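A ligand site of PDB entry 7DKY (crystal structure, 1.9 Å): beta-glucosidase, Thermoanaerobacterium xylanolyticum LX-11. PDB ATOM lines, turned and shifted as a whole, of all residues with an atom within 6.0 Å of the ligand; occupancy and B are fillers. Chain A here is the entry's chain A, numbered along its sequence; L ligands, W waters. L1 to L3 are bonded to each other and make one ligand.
The backbone carbonyl oxygen (O) of Asp 578 sits at hydrogen-bond distance from the indole nitrogen (NE1) of Trp 510 (3.3 Å). NE2 of Gln 712 sits at hydrogen-bond distance from OD1 of Asp 578 (3.1 Å). OH of Tyr 508 is in hydrogen-bond range of OD2 of Asp 578, 2.6 Å away. The side-chain hydroxyl (OH) of Tyr 430 is in hydrogen-bond range of the guanidinium group (NH1) of Arg 771, at 3.1 Å. The side-chain hydroxyl of Tyr 430 lies within hydrogen-bond range of the side-chain hydroxyl of Tyr 47 (2.7 Å). The side-chain amide oxygen of Gln 712 lies within hydrogen-bond range of the backbone NH of Thr 579 (2.9 Å).
Water W2 lies within hydrogen-bond range of OH of Tyr 47 (2.6 Å) and O1 of LG3 L3 (2.8 Å). Water W5 lies within hydrogen-bond range of OG1 of Thr 579, O1 of LG3 L3 and NE2 of Gln 712. Water W3 lies within hydrogen-bond range of the side-chain hydroxyl of Tyr 432 (2.7 Å), an oxygen (O5) of LG3 L3 (2.9 Å), the backbone NH of Asp 509 (3.1 Å) and the backbone NH of Trp 510 (3.3 Å). Water W7 lies within hydrogen-bond range of OH of Tyr 432 and O5 of LG3 L3. Water W6 bridges the guanidinium group of Arg 771 (2.8 Å) and an oxygen (O2) of LG3 L3 (3.4 Å).
Merely in contact with the ligand: Tyr 47, Tyr 430, Tyr 508, Trp 510, Thr 579 and Gln 712. Hydrophobic or aromatic side chains within 4 Å of the ligand: Tyr 47, Tyr 430, Tyr 508 and Trp 510.
OD2 of Asp 578 is in hydrogen-bond range of O3 of LG3 L3 (2.6 Å). NH1 of Arg 771 sits at hydrogen-bond distance from O2 of LG3 L3 (3.1 Å).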
ATOM      1  N   LYS A  46      -5.679  17.288 -14.423  1.00  0.00           N
ATOM      2  CA  LYS A  46      -6.502  16.057 -14.594  1.00  0.00           C
ATOM      3  C   LYS A  46      -7.483  16.121 -15.745  1.00  0.00           C
ATOM      4  O   LYS A  46      -7.965  15.096 -16.219  1.00  0.00           O
ATOM      5  CB  LYS A  46      -7.297  15.789 -13.308  1.00  0.00           C
ATOM      6  CG  LYS A  46      -6.576  14.926 -12.278  1.00  0.00           C
ATOM      7  CD  LYS A  46      -6.955  13.446 -12.391  1.00  0.00           C
ATOM      8  CE  LYS A  46      -6.513  12.634 -11.176  1.00  0.00           C
ATOM      9  NZ  LYS A  46      -7.305  12.880  -9.934  1.00  0.00           N
ATOM     10  N   TYR A  47      -7.792  17.323 -16.212  1.00  0.00           N
ATOM     11  CA  TYR A  47      -8.800  17.555 -17.207  1.00  0.00           C
ATOM     12  C   TYR A  47      -8.102  17.750 -18.555  1.00  0.00           C
ATOM     13  O   TYR A  47      -6.900  17.953 -18.595  1.00  0.00           O
ATOM     14  CB  TYR A  47      -9.672  18.754 -16.849  1.00  0.00           C
ATOM     15  CG  TYR A  47      -8.910  20.037 -16.519  1.00  0.00           C
ATOM     16  CD1 TYR A  47      -8.421  20.272 -15.216  1.00  0.00           C
ATOM     17  CD2 TYR A  47      -8.671  21.013 -17.494  1.00  0.00           C
ATOM     18  CE1 TYR A  47      -7.729  21.451 -14.905  1.00  0.00           C
ATOM     19  CE2 TYR A  47      -7.999  22.191 -17.186  1.00  0.00           C
ATOM     20  CZ  TYR A  47      -7.518  22.403 -15.889  1.00  0.00           C
ATOM     21  OH  TYR A  47      -6.823  23.567 -15.591  1.00  0.00           O
ATOM     22  N   PRO A  48      -8.857  17.666 -19.664  1.00  0.00           N
ATOM     23  CA  PRO A  48      -8.188  17.756 -20.973  1.00  0.00           C
ATOM     24  C   PRO A  48      -7.604  19.139 -21.199  1.00  0.00           C
ATOM     25  O   PRO A  48      -8.196  20.150 -20.801  1.00  0.00           O
ATOM     26  CB  PRO A  48      -9.325  17.463 -21.959  1.00  0.00           C
ATOM     27  CG  PRO A  48     -10.310  16.674 -21.155  1.00  0.00           C
ATOM     28  CD  PRO A  48     -10.272  17.308 -19.807  1.00  0.00           C
ATOM     29  N   TYR A 430      -8.518  28.492 -21.702  1.00  0.00           N
ATOM     30  CA  TYR A 430      -9.438  29.328 -20.972  1.00  0.00           C
ATOM     31  C   TYR A 430      -9.761  30.492 -21.884  1.00  0.00           C
ATOM     32  O   TYR A 430      -9.131  31.561 -21.834  1.00  0.00           O
ATOM     33  CB  TYR A 430      -8.827  29.786 -19.636  1.00  0.00           C
ATOM     34  CG  TYR A 430      -8.065  28.735 -18.844  1.00  0.00           C
ATOM     35  CD1 TYR A 430      -8.538  27.435 -18.706  1.00  0.00           C
ATOM     36  CD2 TYR A 430      -6.911  29.074 -18.161  1.00  0.00           C
ATOM     37  CE1 TYR A 430      -7.830  26.500 -17.939  1.00  0.00           C
ATOM     38  CE2 TYR A 430      -6.216  28.154 -17.384  1.00  0.00           C
ATOM     39  CZ  TYR A 430      -6.675  26.873 -17.280  1.00  0.00           C
ATOM     40  OH  TYR A 430      -5.939  25.988 -16.520  1.00  0.00           O
ATOM     41  N   TYR A 432     -11.018  33.314 -23.108  1.00  0.00           N
ATOM     42  CA  TYR A 432     -11.625  34.606 -22.733  1.00  0.00           C
ATOM     43  C   TYR A 432     -10.798  35.762 -23.289  1.00  0.00           C
ATOM     44  O   TYR A 432      -9.565  35.745 -23.185  1.00  0.00           O
ATOM     45  CB  TYR A 432     -11.726  34.702 -21.189  1.00  0.00           C
ATOM     46  CG  TYR A 432     -12.333  33.463 -20.575  1.00  0.00           C
ATOM     47  CD1 TYR A 432     -13.575  33.034 -21.000  1.00  0.00           C
ATOM     48  CD2 TYR A 432     -11.646  32.670 -19.621  1.00  0.00           C
ATOM     49  CE1 TYR A 432     -14.161  31.887 -20.490  1.00  0.00           C
ATOM     50  CE2 TYR A 432     -12.240  31.501 -19.118  1.00  0.00           C
ATOM     51  CZ  TYR A 432     -13.501  31.126 -19.565  1.00  0.00           C
ATOM     52  OH  TYR A 432     -14.169  29.990 -19.119  1.00  0.00           O
ATOM     53  N   GLY A 476     -18.293  27.729 -10.988  1.00  0.00           N
ATOM     54  CA  GLY A 476     -17.700  26.412 -11.148  1.00  0.00           C
ATOM     55  C   GLY A 476     -17.046  25.841  -9.900  1.00  0.00           C
ATOM     56  O   GLY A 476     -17.116  24.649  -9.665  1.00  0.00           O
ATOM     57  N   TYR A 508     -15.965  34.043 -18.276  1.00  0.00           N
ATOM     58  CA  TYR A 508     -15.349  33.271 -17.207  1.00  0.00           C
ATOM     59  C   TYR A 508     -16.348  32.984 -16.090  1.00  0.00           C
ATOM     60  O   TYR A 508     -17.096  33.894 -15.689  1.00  0.00           O
ATOM     61  CB  TYR A 508     -14.167  34.065 -16.632  1.00  0.00           C
ATOM     62  CG  TYR A 508     -13.505  33.537 -15.386  1.00  0.00           C
ATOM     63  CD1 TYR A 508     -12.495  32.583 -15.451  1.00  0.00           C
ATOM     64  CD2 TYR A 508     -13.840  34.050 -14.129  1.00  0.00           C
ATOM     65  CE1 TYR A 508     -11.855  32.139 -14.294  1.00  0.00           C
ATOM     66  CE2 TYR A 508     -13.209  33.626 -12.983  1.00  0.00           C
ATOM     67  CZ  TYR A 508     -12.229  32.671 -13.053  1.00  0.00           C
ATOM     68  OH  TYR A 508     -11.604  32.277 -11.881  1.00  0.00           O
ATOM     69  N   ASP A 509     -16.335  31.740 -15.600  1.00  0.00           N
ATOM     70  CA  ASP A 509     -17.256  31.311 -14.531  1.00  0.00           C
ATOM     71  C   ASP A 509     -16.683  30.395 -13.444  1.00  0.00           C
ATOM     72  O   ASP A 509     -17.474  29.881 -12.635  1.00  0.00           O
ATOM     73  CB  ASP A 509     -18.520  30.664 -15.160  1.00  0.00           C
ATOM     74  CG  ASP A 509     -18.228  29.360 -15.897  1.00  0.00           C
ATOM     75  OD1 ASP A 509     -17.169  28.743 -15.720  1.00  0.00           O
ATOM     76  OD2 ASP A 509     -19.129  28.922 -16.652  1.00  0.00           O
ATOM     77  N   TRP A 510     -15.374  30.177 -13.412  1.00  0.00           N
ATOM     78  CA  TRP A 510     -14.784  29.320 -12.391  1.00  0.00           C
ATOM     79  C   TRP A 510     -14.916  29.922 -10.984  1.00  0.00           C
ATOM     80  O   TRP A 510     -15.098  29.196 -10.026  1.00  0.00           O
ATOM     81  CB  TRP A 510     -13.328  29.009 -12.716  1.00  0.00           C
ATOM     82  CG  TRP A 510     -12.636  28.277 -11.629  1.00  0.00           C
ATOM     83  CD1 TRP A 510     -11.645  28.768 -10.820  1.00  0.00           C
ATOM     84  CD2 TRP A 510     -12.883  26.937 -11.183  1.00  0.00           C
ATOM     85  NE1 TRP A 510     -11.254  27.820  -9.913  1.00  0.00           N
ATOM     86  CE2 TRP A 510     -12.000  26.685 -10.099  1.00  0.00           C
ATOM     87  CE3 TRP A 510     -13.776  25.932 -11.577  1.00  0.00           C
ATOM     88  CZ2 TRP A 510     -11.980  25.470  -9.423  1.00  0.00           C
ATOM     89  CZ3 TRP A 510     -13.756  24.718 -10.901  1.00  0.00           C
ATOM     90  CH2 TRP A 510     -12.862  24.494  -9.832  1.00  0.00           C
ATOM     91  N   THR A 576      -6.643  36.911  -9.198  1.00  0.00           N
ATOM     92  CA  THR A 576      -6.010  36.182 -10.330  1.00  0.00           C
ATOM     93  C   THR A 576      -5.515  34.780  -9.990  1.00  0.00           C
ATOM     94  O   THR A 576      -5.597  33.874 -10.835  1.00  0.00           O
ATOM     95  CB  THR A 576      -4.898  37.037 -11.009  1.00  0.00           C
ATOM     96  OG1 THR A 576      -4.652  36.574 -12.364  1.00  0.00           O
ATOM     97  CG2 THR A 576      -3.624  37.035 -10.237  1.00  0.00           C
ATOM     98  N   ASP A 578      -6.659  32.072  -8.847  1.00  0.00           N
ATOM     99  CA  ASP A 578      -8.064  31.711  -8.686  1.00  0.00           C
ATOM    100  C   ASP A 578      -8.321  30.293  -8.150  1.00  0.00           C
ATOM    101  O   ASP A 578      -9.471  29.874  -8.092  1.00  0.00           O
ATOM    102  CB  ASP A 578      -8.867  32.016  -9.968  1.00  0.00           C
ATOM    103  CG  ASP A 578      -8.488  31.113 -11.145  1.00  0.00           C
ATOM    104  OD1 ASP A 578      -7.406  30.485 -11.108  1.00  0.00           O
ATOM    105  OD2 ASP A 578      -9.305  31.069 -12.080  1.00  0.00           O
ATOM    106  N   THR A 579      -7.269  29.590  -7.715  1.00  0.00           N
ATOM    107  CA  THR A 579      -7.441  28.466  -6.769  1.00  0.00           C
ATOM    108  C   THR A 579      -6.734  28.694  -5.435  1.00  0.00           C
ATOM    109  O   THR A 579      -6.774  27.832  -4.594  1.00  0.00           O
ATOM    110  CB  THR A 579      -7.085  27.091  -7.375  1.00  0.00           C
ATOM    111  OG1 THR A 579      -5.753  27.086  -7.873  1.00  0.00           O
ATOM    112  CG2 THR A 579      -8.033  26.726  -8.496  1.00  0.00           C
ATOM    113  N   ILE A 711      -2.133  24.126  -5.400  1.00  0.00           N
ATOM    114  CA  ILE A 711      -1.311  23.948  -6.605  1.00  0.00           C
ATOM    115  C   ILE A 711      -0.626  25.230  -7.095  1.00  0.00           C
ATOM    116  O   ILE A 711       0.564  25.200  -7.457  1.00  0.00           O
ATOM    117  CB  ILE A 711      -2.133  23.269  -7.745  1.00  0.00           C
ATOM    118  CG1 ILE A 711      -1.241  22.960  -8.951  1.00  0.00           C
ATOM    119  CG2 ILE A 711      -3.324  24.112  -8.192  1.00  0.00           C
ATOM    120  CD1 ILE A 711      -0.096  22.007  -8.669  1.00  0.00           C
ATOM    121  N   GLN A 712      -1.335  26.352  -7.077  1.00  0.00           N
ATOM    122  CA  GLN A 712      -0.796  27.610  -7.589  1.00  0.00           C
ATOM    123  C   GLN A 712       0.386  28.132  -6.785  1.00  0.00           C
ATOM    124  O   GLN A 712       1.261  28.763  -7.352  1.00  0.00           O
ATOM    125  CB  GLN A 712      -1.874  28.685  -7.717  1.00  0.00           C
ATOM    126  CG  GLN A 712      -2.867  28.348  -8.819  1.00  0.00           C
ATOM    127  CD  GLN A 712      -4.033  29.294  -8.909  1.00  0.00           C
ATOM    128  OE1 GLN A 712      -4.360  30.003  -7.961  1.00  0.00           O
ATOM    129  NE2 GLN A 712      -4.707  29.297 -10.053  1.00  0.00           N
ATOM    130  N   TRP A 717       4.839  30.969 -12.235  1.00  0.00           N
ATOM    131  CA  TRP A 717       4.053  31.635 -13.282  1.00  0.00           C
ATOM    132  C   TRP A 717       5.010  32.455 -14.114  1.00  0.00           C
ATOM    133  O   TRP A 717       5.674  33.373 -13.595  1.00  0.00           O
ATOM    134  CB  TRP A 717       2.942  32.513 -12.696  1.00  0.00           C
ATOM    135  CG  TRP A 717       1.727  31.727 -12.219  1.00  0.00           C
ATOM    136  CD1 TRP A 717       1.657  30.379 -11.987  1.00  0.00           C
ATOM    137  CD2 TRP A 717       0.415  32.249 -11.936  1.00  0.00           C
ATOM    138  NE1 TRP A 717       0.404  30.040 -11.579  1.00  0.00           N
ATOM    139  CE2 TRP A 717      -0.381  31.160 -11.531  1.00  0.00           C
ATOM    140  CE3 TRP A 717      -0.145  33.525 -11.955  1.00  0.00           C
ATOM    141  CZ2 TRP A 717      -1.734  31.304 -11.154  1.00  0.00           C
ATOM    142  CZ3 TRP A 717      -1.507  33.675 -11.588  1.00  0.00           C
ATOM    143  CH2 TRP A 717      -2.277  32.557 -11.204  1.00  0.00           C
ATOM    144  N   ARG A 771       0.880  24.051 -17.208  1.00  0.00           N
ATOM    145  CA  ARG A 771      -0.532  24.374 -17.279  1.00  0.00           C
ATOM    146  C   ARG A 771      -0.748  25.561 -18.239  1.00  0.00           C
ATOM    147  O   ARG A 771      -0.137  26.631 -18.071  1.00  0.00           O
ATOM    148  CB  ARG A 771      -1.119  24.707 -15.901  1.00  0.00           C
ATOM    149  CG  ARG A 771      -2.632  24.880 -15.914  1.00  0.00           C
ATOM    150  CD  ARG A 771      -3.238  24.845 -14.512  1.00  0.00           C
ATOM    151  NE  ARG A 771      -2.726  25.949 -13.701  1.00  0.00           N
ATOM    152  CZ  ARG A 771      -3.211  27.190 -13.675  1.00  0.00           C
ATOM    153  NH1 ARG A 771      -4.253  27.543 -14.398  1.00  0.00           N
ATOM    154  NH2 ARG A 771      -2.654  28.098 -12.871  1.00  0.00           N
HETATM  155  C1  LIG L   1     -13.491  18.291  -9.757  1.00  0.00           C
HETATM  156  C2  LIG L   1     -13.647  19.572 -10.562  1.00  0.00           C
HETATM  157  C3  LIG L   1     -12.686  19.539 -11.748  1.00  0.00           C
HETATM  158  C4  LIG L   1     -12.847  18.280 -12.588  1.00  0.00           C
HETATM  159  C5  LIG L   1     -11.788  18.175 -13.665  1.00  0.00           C
HETATM  160  C6  LIG L   1     -13.694  17.088 -10.673  1.00  0.00           C
HETATM  161  O1  LIG L   1     -13.518  15.917  -9.915  1.00  0.00           O
HETATM  162  O2  LIG L   1     -14.412  18.269  -8.668  1.00  0.00           O
HETATM  163  O3  LIG L   1     -13.398  20.688  -9.704  1.00  0.00           O
HETATM  164  O4  LIG L   1     -12.975  20.646 -12.599  1.00  0.00           O
HETATM  165  O5  LIG L   1     -12.736  17.113 -11.741  1.00  0.00           O
HETATM  166  O6  LIG L   1     -11.768  16.871 -14.233  1.00  0.00           O
HETATM  167  C1  LG2 L   2     -12.466  22.563 -13.871  1.00  0.00           C
HETATM  168  C2  LG2 L   2     -11.338  23.528 -14.268  1.00  0.00           C
HETATM  169  C3  LG2 L   2     -10.592  23.993 -13.017  1.00  0.00           C
HETATM  170  C4  LG2 L   2     -10.161  22.825 -12.137  1.00  0.00           C
HETATM  171  C5  LG2 L   2      -9.568  23.198 -10.782  1.00  0.00           C
HETATM  172  C6  LG2 L   2     -11.913  21.467 -12.968  1.00  0.00           C
HETATM  173  O1  LG2 L   2     -13.070  21.987 -15.018  1.00  0.00           O
HETATM  174  O2  LG2 L   2     -11.893  24.625 -14.984  1.00  0.00           O
HETATM  175  O3  LG2 L   2      -9.406  24.680 -13.462  1.00  0.00           O
HETATM  176  O4  LG2 L   2     -11.317  22.035 -11.829  1.00  0.00           O
HETATM  177  O5  LG2 L   2      -8.905  22.066 -10.217  1.00  0.00           O
HETATM  178  C1  LG3 L   3      -8.027  26.624 -13.199  1.00  0.00           C
HETATM  179  C2  LG3 L   3      -8.081  28.150 -13.185  1.00  0.00           C
HETATM  180  C3  LG3 L   3      -8.724  28.654 -14.477  1.00  0.00           C
HETATM  181  C4  LG3 L   3     -10.110  28.027 -14.624  1.00  0.00           C
HETATM  182  C5  LG3 L   3     -10.814  28.399 -15.916  1.00  0.00           C
HETATM  183  C6  LG3 L   3      -9.429  26.104 -13.414  1.00  0.00           C
HETATM  184  O1  LG3 L   3      -7.480  26.093 -11.994  1.00  0.00           O
HETATM  185  O2  LG3 L   3      -6.777  28.710 -13.011  1.00  0.00           O
HETATM  186  O3  LG3 L   3      -8.830  30.076 -14.479  1.00  0.00           O
HETATM  187  O4  LG3 L   3      -9.974  26.606 -14.617  1.00  0.00           O
HETATM  188  O5  LG3 L   3     -12.115  27.813 -15.980  1.00  0.00           O
HETATM  189  O   HOH W   1     -11.055  21.099  -8.499  1.00  0.00           O
HETATM  190  O   HOH W   2      -6.285  23.808 -13.057  1.00  0.00           O
HETATM  191  O   HOH W   3     -14.283  29.605 -16.441  1.00  0.00           O
HETATM  192  O   HOH W   4      -8.836  19.775 -11.473  1.00  0.00           O
HETATM  193  O   HOH W   5      -5.129  26.285 -10.447  1.00  0.00           O
HETATM  194  O   HOH W   6      -3.938  30.441 -13.676  1.00  0.00           O
HETATM  195  O   HOH W   7     -12.430  27.553 -19.301  1.00  0.00           O
